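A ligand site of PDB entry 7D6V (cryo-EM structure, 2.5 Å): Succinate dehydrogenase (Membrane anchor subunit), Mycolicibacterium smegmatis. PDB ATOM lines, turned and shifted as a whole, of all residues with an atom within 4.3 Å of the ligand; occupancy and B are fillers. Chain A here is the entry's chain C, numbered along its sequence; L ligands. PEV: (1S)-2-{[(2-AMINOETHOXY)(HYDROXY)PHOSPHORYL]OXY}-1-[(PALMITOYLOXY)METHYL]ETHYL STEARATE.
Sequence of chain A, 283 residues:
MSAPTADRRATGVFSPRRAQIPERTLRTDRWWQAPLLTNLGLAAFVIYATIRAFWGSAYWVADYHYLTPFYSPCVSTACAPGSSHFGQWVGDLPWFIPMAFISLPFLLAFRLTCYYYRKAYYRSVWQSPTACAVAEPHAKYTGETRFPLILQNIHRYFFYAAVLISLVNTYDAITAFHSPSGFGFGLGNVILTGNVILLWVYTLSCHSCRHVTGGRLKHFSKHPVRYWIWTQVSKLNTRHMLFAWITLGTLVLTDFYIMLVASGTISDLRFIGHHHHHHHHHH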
ATOM      1  N   LEU A  42      27.068  19.253  15.635  1.00  0.00           N
ATOM      2  CA  LEU A  42      26.360  19.200  14.358  1.00  0.00           C
ATOM      3  C   LEU A  42      27.189  18.502  13.291  1.00  0.00           C
ATOM      4  O   LEU A  42      26.669  17.677  12.530  1.00  0.00           O
ATOM      5  CB  LEU A  42      25.974  20.605  13.917  1.00  0.00           C
ATOM      6  CG  LEU A  42      24.859  21.294  14.690  1.00  0.00           C
ATOM      7  CD1 LEU A  42      24.540  22.652  14.094  1.00  0.00           C
ATOM      8  CD2 LEU A  42      23.614  20.425  14.734  1.00  0.00           C
ATOM      9  N   PHE A  45      27.304  14.670  13.928  1.00  0.00           N
ATOM     10  CA  PHE A  45      26.064  14.007  13.557  1.00  0.00           C
ATOM     11  C   PHE A  45      25.896  13.952  12.048  1.00  0.00           C
ATOM     12  O   PHE A  45      25.488  12.922  11.513  1.00  0.00           O
ATOM     13  CB  PHE A  45      24.851  14.679  14.190  1.00  0.00           C
ATOM     14  CG  PHE A  45      23.549  14.074  13.758  1.00  0.00           C
ATOM     15  CD1 PHE A  45      23.119  12.879  14.307  1.00  0.00           C
ATOM     16  CD2 PHE A  45      22.797  14.660  12.763  1.00  0.00           C
ATOM     17  CE1 PHE A  45      21.932  12.306  13.899  1.00  0.00           C
ATOM     18  CE2 PHE A  45      21.615  14.095  12.346  1.00  0.00           C
ATOM     19  CZ  PHE A  45      21.186  12.912  12.914  1.00  0.00           C
ATOM     20  N   ARG A 111      14.408  19.168  10.812  1.00  0.00           N
ATOM     21  CA  ARG A 111      15.382  19.673  11.779  1.00  0.00           C
ATOM     22  C   ARG A 111      16.095  20.927  11.300  1.00  0.00           C
ATOM     23  O   ARG A 111      16.604  21.686  12.128  1.00  0.00           O
ATOM     24  CB  ARG A 111      16.391  18.581  12.115  1.00  0.00           C
ATOM     25  CG  ARG A 111      15.846  17.562  13.093  1.00  0.00           C
ATOM     26  CD  ARG A 111      16.921  16.666  13.646  1.00  0.00           C
ATOM     27  NE  ARG A 111      16.375  15.619  14.491  1.00  0.00           N
ATOM     28  CZ  ARG A 111      16.465  15.612  15.822  1.00  0.00           C
ATOM     29  NH1 ARG A 111      17.084  16.595  16.449  1.00  0.00           N
ATOM     30  NH2 ARG A 111      15.947  14.619  16.518  1.00  0.00           N
ATOM     31  N   LEU A 112      16.119  21.184   9.988  1.00  0.00           N
ATOM     32  CA  LEU A 112      16.702  22.415   9.485  1.00  0.00           C
ATOM     33  C   LEU A 112      15.800  23.615   9.716  1.00  0.00           C
ATOM     34  O   LEU A 112      16.290  24.733   9.901  1.00  0.00           O
ATOM     35  CB  LEU A 112      17.014  22.268   8.001  1.00  0.00           C
ATOM     36  CG  LEU A 112      18.223  23.041   7.463  1.00  0.00           C
ATOM     37  CD1 LEU A 112      19.495  22.590   8.153  1.00  0.00           C
ATOM     38  CD2 LEU A 112      18.330  22.870   5.969  1.00  0.00           C
ATOM     39  N   THR A 113      14.487  23.409   9.696  1.00  0.00           N
ATOM     40  CA  THR A 113      13.553  24.490   9.960  1.00  0.00           C
ATOM     41  C   THR A 113      13.137  24.579  11.423  1.00  0.00           C
ATOM     42  O   THR A 113      12.355  25.460  11.779  1.00  0.00           O
ATOM     43  CB  THR A 113      12.299  24.341   9.078  1.00  0.00           C
ATOM     44  OG1 THR A 113      11.758  23.032   9.239  1.00  0.00           O
ATOM     45  CG2 THR A 113      12.655  24.562   7.622  1.00  0.00           C
ATOM     46  N   TYR A 117      17.070  24.749  16.246  1.00  0.00           N
ATOM     47  CA  TYR A 117      18.234  24.563  15.388  1.00  0.00           C
ATOM     48  C   TYR A 117      18.566  25.830  14.626  1.00  0.00           C
ATOM     49  O   TYR A 117      19.738  26.119  14.373  1.00  0.00           O
ATOM     50  CB  TYR A 117      17.985  23.407  14.420  1.00  0.00           C
ATOM     51  CG  TYR A 117      18.239  22.053  15.027  1.00  0.00           C
ATOM     52  CD1 TYR A 117      19.536  21.574  15.182  1.00  0.00           C
ATOM     53  CD2 TYR A 117      17.199  21.253  15.446  1.00  0.00           C
ATOM     54  CE1 TYR A 117      19.775  20.331  15.737  1.00  0.00           C
ATOM     55  CE2 TYR A 117      17.423  20.018  16.001  1.00  0.00           C
ATOM     56  CZ  TYR A 117      18.710  19.557  16.147  1.00  0.00           C
ATOM     57  OH  TYR A 117      18.932  18.320  16.689  1.00  0.00           O
ATOM     58  N   TYR A 121      22.387  27.328  14.604  1.00  0.00           N
ATOM     59  CA  TYR A 121      23.314  27.586  13.504  1.00  0.00           C
ATOM     60  C   TYR A 121      23.351  29.050  13.072  1.00  0.00           C
ATOM     61  O   TYR A 121      24.379  29.472  12.563  1.00  0.00           O
ATOM     62  CB  TYR A 121      23.041  26.681  12.292  1.00  0.00           C
ATOM     63  CG  TYR A 121      21.696  26.726  11.618  1.00  0.00           C
ATOM     64  CD1 TYR A 121      20.838  25.634  11.682  1.00  0.00           C
ATOM     65  CD2 TYR A 121      21.290  27.827  10.881  1.00  0.00           C
ATOM     66  CE1 TYR A 121      19.616  25.655  11.058  1.00  0.00           C
ATOM     67  CE2 TYR A 121      20.066  27.856  10.264  1.00  0.00           C
ATOM     68  CZ  TYR A 121      19.232  26.771  10.344  1.00  0.00           C
ATOM     69  OH  TYR A 121      18.010  26.792   9.720  1.00  0.00           O
ATOM     70  N   TYR A 122      22.311  29.847  13.330  1.00  0.00           N
ATOM     71  CA  TYR A 122      22.438  31.291  13.122  1.00  0.00           C
ATOM     72  C   TYR A 122      23.513  31.863  14.027  1.00  0.00           C
ATOM     73  O   TYR A 122      24.230  32.788  13.636  1.00  0.00           O
ATOM     74  CB  TYR A 122      21.110  31.995  13.370  1.00  0.00           C
ATOM     75  CG  TYR A 122      20.071  31.822  12.295  1.00  0.00           C
ATOM     76  CD1 TYR A 122      20.430  31.587  10.977  1.00  0.00           C
ATOM     77  CD2 TYR A 122      18.723  31.905  12.591  1.00  0.00           C
ATOM     78  CE1 TYR A 122      19.481  31.422  10.003  1.00  0.00           C
ATOM     79  CE2 TYR A 122      17.763  31.744  11.624  1.00  0.00           C
ATOM     80  CZ  TYR A 122      18.143  31.498  10.328  1.00  0.00           C
ATOM     81  OH  TYR A 122      17.192  31.341   9.359  1.00  0.00           O
ATOM     82  N   VAL A 125      27.199  29.110  12.715  1.00  0.00           N
ATOM     83  CA  VAL A 125      27.708  29.123  11.345  1.00  0.00           C
ATOM     84  C   VAL A 125      27.586  30.503  10.724  1.00  0.00           C
ATOM     85  O   VAL A 125      28.545  31.027  10.160  1.00  0.00           O
ATOM     86  CB  VAL A 125      26.958  28.059  10.516  1.00  0.00           C
ATOM     87  CG1 VAL A 125      27.528  27.985   9.111  1.00  0.00           C
ATOM     88  CG2 VAL A 125      27.017  26.715  11.206  1.00  0.00           C
ATOM     89  N   TRP A 126      26.404  31.102  10.816  1.00  0.00           N
ATOM     90  CA  TRP A 126      26.162  32.388  10.186  1.00  0.00           C
ATOM     91  C   TRP A 126      26.639  33.558  11.031  1.00  0.00           C
ATOM     92  O   TRP A 126      26.689  34.682  10.534  1.00  0.00           O
ATOM     93  CB  TRP A 126      24.674  32.545   9.864  1.00  0.00           C
ATOM     94  CG  TRP A 126      24.349  33.649   8.893  1.00  0.00           C
ATOM     95  CD1 TRP A 126      23.400  34.611   9.039  1.00  0.00           C
ATOM     96  CD2 TRP A 126      24.969  33.891   7.621  1.00  0.00           C
ATOM     97  NE1 TRP A 126      23.391  35.441   7.949  1.00  0.00           N
ATOM     98  CE2 TRP A 126      24.353  35.026   7.067  1.00  0.00           C
ATOM     99  CE3 TRP A 126      25.996  33.264   6.908  1.00  0.00           C
ATOM    100  CZ2 TRP A 126      24.713  35.540   5.831  1.00  0.00           C
ATOM    101  CZ3 TRP A 126      26.356  33.786   5.677  1.00  0.00           C
ATOM    102  CH2 TRP A 126      25.719  34.908   5.152  1.00  0.00           C
ATOM    103  N   LYS A 140      25.388  44.097   6.410  1.00  0.00           N
ATOM    104  CA  LYS A 140      23.965  44.135   6.148  1.00  0.00           C
ATOM    105  C   LYS A 140      23.288  42.940   6.814  1.00  0.00           C
ATOM    106  O   LYS A 140      23.911  41.911   7.056  1.00  0.00           O
ATOM    107  CB  LYS A 140      23.684  44.116   4.643  1.00  0.00           C
ATOM    108  CG  LYS A 140      24.246  45.327   3.905  1.00  0.00           C
ATOM    109  CD  LYS A 140      23.534  46.593   4.324  1.00  0.00           C
ATOM    110  CE  LYS A 140      24.021  47.795   3.542  1.00  0.00           C
ATOM    111  NZ  LYS A 140      23.338  49.040   3.998  1.00  0.00           N
ATOM    112  N   TYR A 141      21.999  43.098   7.112  1.00  0.00           N
ATOM    113  CA  TYR A 141      21.240  42.036   7.762  1.00  0.00           C
ATOM    114  C   TYR A 141      19.768  42.197   7.422  1.00  0.00           C
ATOM    115  O   TYR A 141      19.194  43.255   7.703  1.00  0.00           O
ATOM    116  CB  TYR A 141      21.452  42.064   9.270  1.00  0.00           C
ATOM    117  CG  TYR A 141      20.534  41.143  10.041  1.00  0.00           C
ATOM    118  CD1 TYR A 141      20.810  39.798  10.164  1.00  0.00           C
ATOM    119  CD2 TYR A 141      19.385  41.644  10.649  1.00  0.00           C
ATOM    120  CE1 TYR A 141      19.971  38.967  10.872  1.00  0.00           C
ATOM    121  CE2 TYR A 141      18.551  40.822  11.347  1.00  0.00           C
ATOM    122  CZ  TYR A 141      18.846  39.484  11.465  1.00  0.00           C
ATOM    123  OH  TYR A 141      18.001  38.666  12.170  1.00  0.00           O
ATOM    124  N   THR A 142      19.173  41.174   6.822  1.00  0.00           N
ATOM    125  CA  THR A 142      17.746  41.185   6.545  1.00  0.00           C
ATOM    126  C   THR A 142      16.955  40.201   7.404  1.00  0.00           C
ATOM    127  O   THR A 142      15.731  40.313   7.458  1.00  0.00           O
ATOM    128  CB  THR A 142      17.493  40.867   5.058  1.00  0.00           C
ATOM    129  OG1 THR A 142      17.796  39.501   4.791  1.00  0.00           O
ATOM    130  CG2 THR A 142      18.343  41.750   4.183  1.00  0.00           C
ATOM    131  N   GLY A 143      17.626  39.280   8.076  1.00  0.00           N
ATOM    132  CA  GLY A 143      16.916  38.341   8.932  1.00  0.00           C
ATOM    133  C   GLY A 143      16.254  37.255   8.108  1.00  0.00           C
ATOM    134  O   GLY A 143      16.882  36.638   7.249  1.00  0.00           O
ATOM    135  N   ARG A 146      13.885  37.785   3.342  1.00  0.00           N
ATOM    136  CA  ARG A 146      14.163  37.624   1.918  1.00  0.00           C
ATOM    137  C   ARG A 146      13.970  36.175   1.499  1.00  0.00           C
ATOM    138  O   ARG A 146      13.732  35.287   2.321  1.00  0.00           O
ATOM    139  CB  ARG A 146      15.567  38.117   1.593  1.00  0.00           C
ATOM    140  CG  ARG A 146      15.843  39.535   2.027  1.00  0.00           C
ATOM    141  CD  ARG A 146      15.609  40.508   0.900  1.00  0.00           C
ATOM    142  NE  ARG A 146      15.695  41.891   1.361  1.00  0.00           N
ATOM    143  CZ  ARG A 146      16.560  42.776   0.879  1.00  0.00           C
ATOM    144  NH1 ARG A 146      16.578  44.014   1.361  1.00  0.00           N
ATOM    145  NH2 ARG A 146      17.427  42.419  -0.058  1.00  0.00           N
ATOM    146  N   PRO A 148      15.451  33.217   0.417  1.00  0.00           N
ATOM    147  CA  PRO A 148      15.881  31.931   0.999  1.00  0.00           C
ATOM    148  C   PRO A 148      15.354  31.711   2.404  1.00  0.00           C
ATOM    149  O   PRO A 148      14.710  30.692   2.672  1.00  0.00           O
ATOM    150  CB  PRO A 148      17.412  32.021   0.949  1.00  0.00           C
ATOM    151  CG  PRO A 148      17.721  33.455   0.859  1.00  0.00           C
ATOM    152  CD  PRO A 148      16.604  34.085   0.110  1.00  0.00           C
ATOM    153  N   LEU A 149      15.585  32.654   3.313  1.00  0.00           N
ATOM    154  CA  LEU A 149      15.252  32.452   4.718  1.00  0.00           C
ATOM    155  C   LEU A 149      13.785  32.704   5.040  1.00  0.00           C
ATOM    156  O   LEU A 149      13.355  32.351   6.143  1.00  0.00           O
ATOM    157  CB  LEU A 149      16.135  33.354   5.582  1.00  0.00           C
ATOM    158  CG  LEU A 149      17.610  32.948   5.638  1.00  0.00           C
ATOM    159  CD1 LEU A 149      18.338  33.684   6.751  1.00  0.00           C
ATOM    160  CD2 LEU A 149      17.745  31.448   5.828  1.00  0.00           C
ATOM    161  N   LEU A 151      11.583  31.025   3.749  1.00  0.00           N
ATOM    162  CA  LEU A 151      11.023  29.690   3.632  1.00  0.00           C
ATOM    163  C   LEU A 151      11.044  28.922   4.948  1.00  0.00           C
ATOM    164  O   LEU A 151      10.515  27.804   4.991  1.00  0.00           O
ATOM    165  CB  LEU A 151      11.789  28.901   2.567  1.00  0.00           C
ATOM    166  CG  LEU A 151      11.645  29.377   1.132  1.00  0.00           C
ATOM    167  CD1 LEU A 151      12.569  28.594   0.208  1.00  0.00           C
ATOM    168  CD2 LEU A 151      10.211  29.254   0.659  1.00  0.00           C
ATOM    169  N   GLN A 152      11.632  29.477   6.008  1.00  0.00           N
ATOM    170  CA  GLN A 152      11.604  28.816   7.301  1.00  0.00           C
ATOM    171  C   GLN A 152      10.212  28.811   7.926  1.00  0.00           C
ATOM    172  O   GLN A 152      10.021  28.164   8.965  1.00  0.00           O
ATOM    173  CB  GLN A 152      12.582  29.493   8.258  1.00  0.00           C
ATOM    174  CG  GLN A 152      13.978  29.679   7.681  1.00  0.00           C
ATOM    175  CD  GLN A 152      14.908  28.568   8.071  1.00  0.00           C
ATOM    176  OE1 GLN A 152      14.491  27.426   8.246  1.00  0.00           O
ATOM    177  NE2 GLN A 152      16.194  28.887   8.203  1.00  0.00           N
ATOM    178  N   LEU A 248      19.355  13.262  18.799  1.00  0.00           N
ATOM    179  CA  LEU A 248      20.506  13.044  17.928  1.00  0.00           C
ATOM    180  C   LEU A 248      21.406  11.941  18.469  1.00  0.00           C
ATOM    181  O   LEU A 248      21.789  11.006  17.746  1.00  0.00           O
ATOM    182  CB  LEU A 248      21.298  14.342  17.770  1.00  0.00           C
ATOM    183  CG  LEU A 248      20.710  15.432  16.877  1.00  0.00           C
ATOM    184  CD1 LEU A 248      21.776  16.419  16.470  1.00  0.00           C
ATOM    185  CD2 LEU A 248      20.037  14.815  15.655  1.00  0.00           C
HETATM  186  C48 PEV L   1      20.391  17.331  13.145  1.00  0.00           C
HETATM  187  C47 PEV L   1      20.569  17.497  11.643  1.00  0.00           C
HETATM  188  C46 PEV L   1      20.329  18.940  11.227  1.00  0.00           C
HETATM  189  C45 PEV L   1      21.559  19.789  11.514  1.00  0.00           C
HETATM  190  C44 PEV L   1      21.718  20.900  10.486  1.00  0.00           C
HETATM  191  C43 PEV L   1      22.671  21.982  10.974  1.00  0.00           C
HETATM  192  C42 PEV L   1      23.535  22.504   9.839  1.00  0.00           C
HETATM  193  C41 PEV L   1      23.043  23.861   9.347  1.00  0.00           C
HETATM  194  C40 PEV L   1      24.144  24.624   8.639  1.00  0.00           C
HETATM  195  C39 PEV L   1      23.619  25.264   7.365  1.00  0.00           C
HETATM  196  C38 PEV L   1      22.837  26.532   7.693  1.00  0.00           C
HETATM  197  C37 PEV L   1      23.765  27.742   7.744  1.00  0.00           C
HETATM  198  C36 PEV L   1      23.219  28.876   6.907  1.00  0.00           C
HETATM  199  C35 PEV L   1      22.475  29.889   7.778  1.00  0.00           C
HETATM  200  C34 PEV L   1      22.527  31.267   7.143  1.00  0.00           C
HETATM  201  C33 PEV L   1      22.117  31.212   5.683  1.00  0.00           C
HETATM  202  C32 PEV L   1      22.746  32.368   4.901  1.00  0.00           C
HETATM  203  C31 PEV L   1      21.795  33.549   4.837  1.00  0.00           C
HETATM  204  O31 PEV L   1      21.500  34.117   5.826  1.00  0.00           O
HETATM  205  O2  PEV L   1      21.286  33.960   3.605  1.00  0.00           O
HETATM  206  C2  PEV L   1      21.771  35.202   3.211  1.00  0.00           C
HETATM  207  C1  PEV L   1      20.713  36.253   3.548  1.00  0.00           C
HETATM  208  O3P PEV L   1      20.987  36.760   4.819  1.00  0.00           O
HETATM  209  P   PEV L   1      21.334  38.364   4.971  1.00  0.00           P
HETATM  210  O1P PEV L   1      22.780  38.617   4.642  1.00  0.00           O
HETATM  211  O2P PEV L   1      21.057  38.792   6.393  1.00  0.00           O
HETATM  212  O4P PEV L   1      20.386  39.207   3.931  1.00  0.00           O
HETATM  213  C4  PEV L   1      20.950  39.653   2.726  1.00  0.00           C
HETATM  214  C5  PEV L   1      19.884  39.536   1.636  1.00  0.00           C
HETATM  215  N6  PEV L   1      20.518  39.472   0.320  1.00  0.00           N
HETATM  216  C3  PEV L   1      22.051  35.180   1.720  1.00  0.00           C
HETATM  217  O3  PEV L   1      22.790  34.026   1.447  1.00  0.00           O
HETATM  218  C11 PEV L   1      22.102  33.059   0.711  1.00  0.00           C
HETATM  219  O11 PEV L   1      21.712  33.301  -0.378  1.00  0.00           O
HETATM  220  C12 PEV L   1      21.830  31.687   1.325  1.00  0.00           C
HETATM  221  C13 PEV L   1      22.177  30.552   0.366  1.00  0.00           C
HETATM  222  C14 PEV L   1      22.395  29.232   1.104  1.00  0.00           C
HETATM  223  C15 PEV L   1      21.282  28.920   2.087  1.00  0.00           C
HETATM  224  C16 PEV L   1      20.589  27.602   1.754  1.00  0.00           C
HETATM  225  C17 PEV L   1      20.235  26.769   2.981  1.00  0.00           C
HETATM  226  C18 PEV L   1      20.568  27.444   4.315  1.00  0.00           C
HETATM  227  C19 PEV L   1      19.363  27.560   5.240  1.00  0.00           C
HETATM  228  C20 PEV L   1      18.048  27.145   4.598  1.00  0.00           C
HETATM  229  C21 PEV L   1      16.987  26.793   5.633  1.00  0.00           C
HETATM  230  C22 PEV L   1      15.882  25.911   5.053  1.00  0.00           C
HETATM  231  C23 PEV L   1      14.666  26.706   4.563  1.00  0.00           C
HETATM  232  C24 PEV L   1      14.085  26.086   3.304  1.00  0.00           C
HETATM  233  C25 PEV L   1      13.198  24.891   3.602  1.00  0.00           C
HETATM  234  C26 PEV L   1      13.693  23.627   2.911  1.00  0.00           C
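An oxygen (O2P) of the ligand sits at hydrogen-bond distance from the backbone NH (N) of Thr 142 (3.1 Å).
The side-chain hydroxyl (OG1) of Thr 142 is in hydrogen-bond range of an oxygen (O4P) of the ligand (2.7 Å).
NE1 of Trp 126 lies within hydrogen-bond range of O31 of the ligand, 3.1 Å away.
N of Trp 126 lies within hydrogen-bond range of O of Tyr 121 (3.1 Å).
The side-chain amide nitrogen (NE2) of Gln 152 sits at hydrogen-bond distance from the side-chain hydroxyl (OH) of Tyr 121 (3.2 Å).
NE2 of Gln 152 sits at hydrogen-bond distance from OH of Tyr 122.
The guanidinium group of Arg 111 lies within hydrogen-bond range of the side-chain hydroxyl of Tyr 117, at 2.5 Å.
The side-chain hydroxyl (OH) of Tyr 121 is in hydrogen-bond range of the backbone carbonyl oxygen (O) of Leu 112 (2.7 Å).
Leu 42 touches the ligand.
CE2 of Phe 45 touches C48 of the ligand, 3.6 Å away.
Arg 111 touches the ligand (CD to C48, 3.6 Å).
Leu 112 touches the ligand (CD1 to C44, 3.6 Å).
OH of Tyr 117 touches C48 of the ligand (3.96 Å).
Tyr 121 touches the ligand.
Tyr 141 touches the ligand.
N of Gly 143 touches O2P of the ligand, 3.9 Å away.
CD1 of Leu 149 touches O31 of the ligand (3.3 Å).
Leu 151 touches the ligand.
Gln 152 touches the ligand.
Leu 248 touches the ligand (CD2 to C48, 3.6 Å).
Hydrophobic or aromatic side chains that line the ligand: Leu 42, Phe 45, Leu 112, Tyr 121, Trp 126, Tyr 141, Leu 149, Leu 151 and Leu 248.
Of the 20 residues printed, 14 come within 4 Å of the ligand.
The nearest printed residue that does not touch the ligand is Val 125 (4.01 Å).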
